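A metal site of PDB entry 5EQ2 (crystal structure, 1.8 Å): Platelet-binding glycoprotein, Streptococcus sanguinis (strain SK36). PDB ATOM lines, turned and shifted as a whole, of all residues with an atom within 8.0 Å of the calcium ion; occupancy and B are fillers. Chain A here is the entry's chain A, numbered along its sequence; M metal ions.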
ATOM      1  N   ARG A   2      -7.042  10.681  -3.729  1.00  0.00           N
ATOM      2  CA  ARG A   2      -8.118   9.732  -3.952  1.00  0.00           C
ATOM      3  C   ARG A   2      -8.394   8.947  -2.672  1.00  0.00           C
ATOM      4  O   ARG A   2      -7.460   8.548  -1.970  1.00  0.00           O
ATOM      5  CB  ARG A   2      -7.769   8.779  -5.096  1.00  0.00           C
ATOM      6  CG  ARG A   2      -7.202   9.478  -6.333  1.00  0.00           C
ATOM      7  CD  ARG A   2      -6.316   8.545  -7.156  1.00  0.00           C
ATOM      8  NE  ARG A   2      -4.964   8.451  -6.606  1.00  0.00           N
ATOM      9  CZ  ARG A   2      -4.469   7.380  -6.003  1.00  0.00           C
ATOM     10  NH1 ARG A   2      -5.219   6.284  -5.859  1.00  0.00           N
ATOM     11  NH2 ARG A   2      -3.223   7.384  -5.540  1.00  0.00           N
ATOM     12  N   THR A   4      -9.256   6.045  -2.048  1.00  0.00           N
ATOM     13  CA  THR A   4      -8.968   4.630  -1.983  1.00  0.00           C
ATOM     14  C   THR A   4      -7.778   4.265  -2.855  1.00  0.00           C
ATOM     15  O   THR A   4      -7.474   4.927  -3.857  1.00  0.00           O
ATOM     16  CB  THR A   4     -10.187   3.791  -2.400  1.00  0.00           C
ATOM     17  OG1 THR A   4     -10.652   4.236  -3.686  1.00  0.00           O
ATOM     18  CG2 THR A   4     -11.313   3.919  -1.385  1.00  0.00           C
ATOM     19  N   ASP A   5      -7.092   3.208  -2.430  1.00  0.00           N
ATOM     20  CA  ASP A   5      -6.078   2.525  -3.233  1.00  0.00           C
ATOM     21  C   ASP A   5      -6.759   1.554  -4.180  1.00  0.00           C
ATOM     22  O   ASP A   5      -7.397   0.583  -3.745  1.00  0.00           O
ATOM     23  CB  ASP A   5      -5.123   1.814  -2.275  1.00  0.00           C
ATOM     24  CG  ASP A   5      -3.932   1.182  -2.981  1.00  0.00           C
ATOM     25  OD1 ASP A   5      -3.977   1.009  -4.211  1.00  0.00           O
ATOM     26  OD2 ASP A   5      -2.945   0.857  -2.269  1.00  0.00           O
ATOM     27  N   THR A   6      -6.647   1.809  -5.480  1.00  0.00           N
ATOM     28  CA  THR A   6      -7.214   0.906  -6.469  1.00  0.00           C
ATOM     29  C   THR A   6      -6.162   0.357  -7.410  1.00  0.00           C
ATOM     30  O   THR A   6      -6.512  -0.275  -8.415  1.00  0.00           O
ATOM     31  CB  THR A   6      -8.286   1.625  -7.272  1.00  0.00           C
ATOM     32  OG1 THR A   6      -7.680   2.734  -7.943  1.00  0.00           O
ATOM     33  CG2 THR A   6      -9.393   2.123  -6.345  1.00  0.00           C
ATOM     34  N   THR A   7      -4.881   0.568  -7.111  1.00  0.00           N
ATOM     35  CA  THR A   7      -3.776   0.183  -7.988  1.00  0.00           C
ATOM     36  C   THR A   7      -3.008  -0.993  -7.394  1.00  0.00           C
ATOM     37  O   THR A   7      -2.521  -0.896  -6.255  1.00  0.00           O
ATOM     38  CB  THR A   7      -2.848   1.397  -8.149  1.00  0.00           C
ATOM     39  OG1 THR A   7      -3.624   2.527  -8.593  1.00  0.00           O
ATOM     40  CG2 THR A   7      -1.703   1.147  -9.147  1.00  0.00           C
ATOM     41  N   PRO A   8      -2.820  -2.074  -8.128  1.00  0.00           N
ATOM     42  CA  PRO A   8      -2.101  -3.215  -7.564  1.00  0.00           C
ATOM     43  C   PRO A   8      -0.600  -2.969  -7.567  1.00  0.00           C
ATOM     44  O   PRO A   8      -0.110  -2.028  -8.204  1.00  0.00           O
ATOM     45  CB  PRO A   8      -2.482  -4.364  -8.513  1.00  0.00           C
ATOM     46  CG  PRO A   8      -2.703  -3.708  -9.824  1.00  0.00           C
ATOM     47  CD  PRO A   8      -3.324  -2.356  -9.486  1.00  0.00           C
ATOM     48  N   PRO A   9       0.144  -3.804  -6.862  1.00  0.00           N
ATOM     49  CA  PRO A   9       1.612  -3.705  -6.843  1.00  0.00           C
ATOM     50  C   PRO A   9       2.223  -3.937  -8.224  1.00  0.00           C
ATOM     51  O   PRO A   9       1.601  -4.503  -9.122  1.00  0.00           O
ATOM     52  CB  PRO A   9       2.041  -4.834  -5.895  1.00  0.00           C
ATOM     53  CG  PRO A   9       0.856  -5.095  -5.038  1.00  0.00           C
ATOM     54  CD  PRO A   9      -0.357  -4.829  -5.918  1.00  0.00           C
ATOM     55  N   THR A  10       3.459  -3.492  -8.355  1.00  0.00           N
ATOM     56  CA  THR A  10       4.262  -3.641  -9.563  1.00  0.00           C
ATOM     57  C   THR A  10       5.446  -4.544  -9.262  1.00  0.00           C
ATOM     58  O   THR A  10       6.179  -4.282  -8.313  1.00  0.00           O
ATOM     59  CB  THR A  10       4.773  -2.259 -10.015  1.00  0.00           C
ATOM     60  OG1 THR A  10       3.649  -1.418 -10.317  1.00  0.00           O
ATOM     61  CG2 THR A  10       5.620  -2.390 -11.250  1.00  0.00           C
ATOM     62  N   THR A  32       6.957  -3.105  -5.629  1.00  0.00           N
ATOM     63  CA  THR A  32       6.574  -1.825  -5.034  1.00  0.00           C
ATOM     64  C   THR A  32       5.062  -1.684  -5.111  1.00  0.00           C
ATOM     65  O   THR A  32       4.404  -2.326  -5.922  1.00  0.00           O
ATOM     66  CB  THR A  32       7.221  -0.641  -5.741  1.00  0.00           C
ATOM     67  OG1 THR A  32       6.725  -0.562  -7.077  1.00  0.00           O
ATOM     68  CG2 THR A  32       8.743  -0.802  -5.776  1.00  0.00           C
ATOM     69  N   ASP A  33       4.513  -0.834  -4.255  1.00  0.00           N
ATOM     70  CA  ASP A  33       3.102  -0.475  -4.357  1.00  0.00           C
ATOM     71  C   ASP A  33       2.949   0.996  -4.019  1.00  0.00           C
ATOM     72  O   ASP A  33       3.687   1.538  -3.183  1.00  0.00           O
ATOM     73  CB  ASP A  33       2.218  -1.313  -3.433  1.00  0.00           C
ATOM     74  CG  ASP A  33       0.731  -1.044  -3.647  1.00  0.00           C
ATOM     75  OD1 ASP A  33       0.209  -1.459  -4.689  1.00  0.00           O
ATOM     76  OD2 ASP A  33       0.102  -0.406  -2.774  1.00  0.00           O
ATOM     77  N   ASP A  34       1.957   1.654  -4.645  1.00  0.00           N
ATOM     78  CA  ASP A  34       1.753   3.074  -4.363  1.00  0.00           C
ATOM     79  C   ASP A  34       1.460   3.359  -2.892  1.00  0.00           C
ATOM     80  O   ASP A  34       1.762   4.441  -2.402  1.00  0.00           O
ATOM     81  CB  ASP A  34       0.642   3.657  -5.277  1.00  0.00           C
ATOM     82  CG  ASP A  34      -0.742   2.984  -5.083  1.00  0.00           C
ATOM     83  OD1 ASP A  34      -0.840   1.770  -4.748  1.00  0.00           O
ATOM     84  OD2 ASP A  34      -1.761   3.692  -5.311  1.00  0.00           O
ATOM     85  N   SER A  35       0.934   2.377  -2.154  1.00  0.00           N
ATOM     86  CA  SER A  35       0.703   2.486  -0.716  1.00  0.00           C
ATOM     87  C   SER A  35       1.963   2.295   0.105  1.00  0.00           C
ATOM     88  O   SER A  35       1.967   2.622   1.303  1.00  0.00           O
ATOM     89  CB  SER A  35      -0.299   1.428  -0.254  1.00  0.00           C
ATOM     90  OG  SER A  35       0.325   0.138  -0.237  1.00  0.00           O
ATOM     91  N   GLY A  36       2.996   1.705  -0.482  1.00  0.00           N
ATOM     92  CA  GLY A  36       4.185   1.366   0.253  1.00  0.00           C
ATOM     93  C   GLY A  36       4.138   0.033   0.969  1.00  0.00           C
ATOM     94  O   GLY A  36       5.107  -0.312   1.647  1.00  0.00           O
ATOM     95  N   GLN A  37       3.050  -0.726   0.839  1.00  0.00           N
ATOM     96  CA  GLN A  37       2.859  -1.962   1.593  1.00  0.00           C
ATOM     97  C   GLN A  37       2.389  -3.067   0.659  1.00  0.00           C
ATOM     98  O   GLN A  37       1.318  -2.949   0.052  1.00  0.00           O
ATOM     99  CB  GLN A  37       1.851  -1.784   2.727  1.00  0.00           C
ATOM    100  CG  GLN A  37       1.722  -3.050   3.603  1.00  0.00           C
ATOM    101  CD  GLN A  37       0.904  -2.809   4.862  1.00  0.00           C
ATOM    102  OE1 GLN A  37       0.697  -1.654   5.258  1.00  0.00           O
ATOM    103  NE2 GLN A  37       0.394  -3.868   5.457  1.00  0.00           N
ATOM    104  N   VAL A  38       3.165  -4.157   0.588  1.00  0.00           N
ATOM    105  CA  VAL A  38       2.769  -5.374  -0.124  1.00  0.00           C
ATOM    106  C   VAL A  38       2.413  -6.429   0.899  1.00  0.00           C
ATOM    107  O   VAL A  38       3.168  -6.638   1.854  1.00  0.00           O
ATOM    108  CB  VAL A  38       3.890  -5.836  -1.068  1.00  0.00           C
ATOM    109  CG1 VAL A  38       3.711  -7.286  -1.551  1.00  0.00           C
ATOM    110  CG2 VAL A  38       3.978  -4.886  -2.274  1.00  0.00           C
ATOM    111  N   TRP A 104      -0.346  -8.999  -3.918  1.00  0.00           N
ATOM    112  CA  TRP A 104      -1.448  -8.238  -3.320  1.00  0.00           C
ATOM    113  C   TRP A 104      -0.893  -7.067  -2.524  1.00  0.00           C
ATOM    114  O   TRP A 104       0.117  -7.209  -1.831  1.00  0.00           O
ATOM    115  CB  TRP A 104      -2.234  -9.109  -2.324  1.00  0.00           C
ATOM    116  CG  TRP A 104      -3.180 -10.127  -2.914  1.00  0.00           C
ATOM    117  CD1 TRP A 104      -4.544 -10.021  -2.999  1.00  0.00           C
ATOM    118  CD2 TRP A 104      -2.838 -11.412  -3.447  1.00  0.00           C
ATOM    119  NE1 TRP A 104      -5.076 -11.157  -3.570  1.00  0.00           N
ATOM    120  CE2 TRP A 104      -4.052 -12.024  -3.863  1.00  0.00           C
ATOM    121  CE3 TRP A 104      -1.635 -12.122  -3.606  1.00  0.00           C
ATOM    122  CZ2 TRP A 104      -4.098 -13.285  -4.438  1.00  0.00           C
ATOM    123  CZ3 TRP A 104      -1.670 -13.376  -4.199  1.00  0.00           C
ATOM    124  CH2 TRP A 104      -2.898 -13.952  -4.589  1.00  0.00           C
ATOM    125  N   ASP A 105      -1.603  -5.932  -2.550  1.00  0.00           N
ATOM    126  CA  ASP A 105      -1.353  -4.899  -1.559  1.00  0.00           C
ATOM    127  C   ASP A 105      -2.300  -5.119  -0.378  1.00  0.00           C
ATOM    128  O   ASP A 105      -2.991  -6.134  -0.312  1.00  0.00           O
ATOM    129  CB  ASP A 105      -1.461  -3.502  -2.184  1.00  0.00           C
ATOM    130  CG  ASP A 105      -2.867  -3.142  -2.651  1.00  0.00           C
ATOM    131  OD1 ASP A 105      -3.861  -3.802  -2.246  1.00  0.00           O
ATOM    132  OD2 ASP A 105      -2.981  -2.161  -3.416  1.00  0.00           O
ATOM    133  N   ALA A 106      -2.298  -4.211   0.595  1.00  0.00           N
ATOM    134  CA  ALA A 106      -3.123  -4.373   1.790  1.00  0.00           C
ATOM    135  C   ALA A 106      -4.558  -3.910   1.589  1.00  0.00           C
ATOM    136  O   ALA A 106      -5.350  -4.011   2.522  1.00  0.00           O
ATOM    137  CB  ALA A 106      -2.507  -3.600   2.956  1.00  0.00           C
ATOM    138  N   ALA A 107      -4.887  -3.388   0.410  1.00  0.00           N
ATOM    139  CA  ALA A 107      -6.231  -2.938   0.086  1.00  0.00           C
ATOM    140  C   ALA A 107      -6.982  -3.947  -0.770  1.00  0.00           C
ATOM    141  O   ALA A 107      -8.075  -3.660  -1.248  1.00  0.00           O
ATOM    142  CB  ALA A 107      -6.170  -1.584  -0.630  1.00  0.00           C
ATOM    143  N   GLY A 108      -6.385  -5.115  -1.013  1.00  0.00           N
ATOM    144  CA  GLY A 108      -7.035  -6.157  -1.763  1.00  0.00           C
ATOM    145  C   GLY A 108      -6.809  -6.094  -3.252  1.00  0.00           C
ATOM    146  O   GLY A 108      -7.410  -6.900  -3.980  1.00  0.00           O
ATOM    147  N   ASN A 109      -5.983  -5.182  -3.739  1.00  0.00           N
ATOM    148  CA  ASN A 109      -5.659  -5.152  -5.157  1.00  0.00           C
ATOM    149  C   ASN A 109      -4.586  -6.194  -5.454  1.00  0.00           C
ATOM    150  O   ASN A 109      -3.531  -6.204  -4.813  1.00  0.00           O
ATOM    151  CB  ASN A 109      -5.150  -3.756  -5.550  1.00  0.00           C
ATOM    152  CG  ASN A 109      -6.146  -2.673  -5.211  1.00  0.00           C
ATOM    153  OD1 ASN A 109      -7.247  -2.632  -5.755  1.00  0.00           O
ATOM    154  ND2 ASN A 109      -5.768  -1.779  -4.305  1.00  0.00           N
ATOM    155  N   VAL A 110      -4.825  -7.049  -6.464  1.00  0.00           N
ATOM    156  CA  VAL A 110      -3.855  -8.065  -6.839  1.00  0.00           C
ATOM    157  C   VAL A 110      -3.383  -7.765  -8.260  1.00  0.00           C
ATOM    158  O   VAL A 110      -4.178  -7.369  -9.125  1.00  0.00           O
ATOM    159  CB  VAL A 110      -4.407  -9.493  -6.710  1.00  0.00           C
ATOM    160  CG1 VAL A 110      -5.612  -9.724  -7.630  1.00  0.00           C
ATOM    161  CG2 VAL A 110      -3.336 -10.528  -6.995  1.00  0.00           C
HETATM  162 CA    CA M   1      -1.875  -0.260  -4.220  1.00  0.00          CA
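The side-chain amide nitrogen of Asn 109 sits at hydrogen-bond distance from the backbone carbonyl oxygen of Asp 5 (2.9 Å).
The backbone NH (N) of Ala 107 lies within hydrogen-bond range of the side-chain carboxylate (OD1) of Asp 105.
The guanidinium group (NH2) of Arg 2 is in salt-bridge range of the side-chain carboxylate (OD2) of Asp 34.
The side-chain carboxylate (OD2) of Asp 33 sits close to the side-chain hydroxyl (OG) of Ser 35 (2.6 Å).
The side-chain carboxylate (OD1) of Asp 105 sits at hydrogen-bond distance from the backbone NH (N) of Asn 109 (2.9 Å).
OD1 of Asp 105 sits at hydrogen-bond distance from N of Gly 108, at 3.1 Å.
Five residues have an atom within 4 Å of the calcium ion: Asp 5, Thr 7, Asp 33, Asp 34 and Asp 105.
O of Thr 7 binds the calcium ion (2.2 Å).
The calcium ion is bound by OD1 of Asp 34 (2.3 Å).
The side-chain carboxylate (OD2) of Asp 105 is bound to the calcium ion, at 2.3 Å.
OD1 of Asp 33 binds the calcium ion, at 2.4 Å.
The calcium ion is bound by the side-chain carboxylate (OD2) of Asp 33, 2.5 Å away.
The calcium ion is bound by OD1 of Asp 5.
The calcium ion is bound by OD2 of Asp 5.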
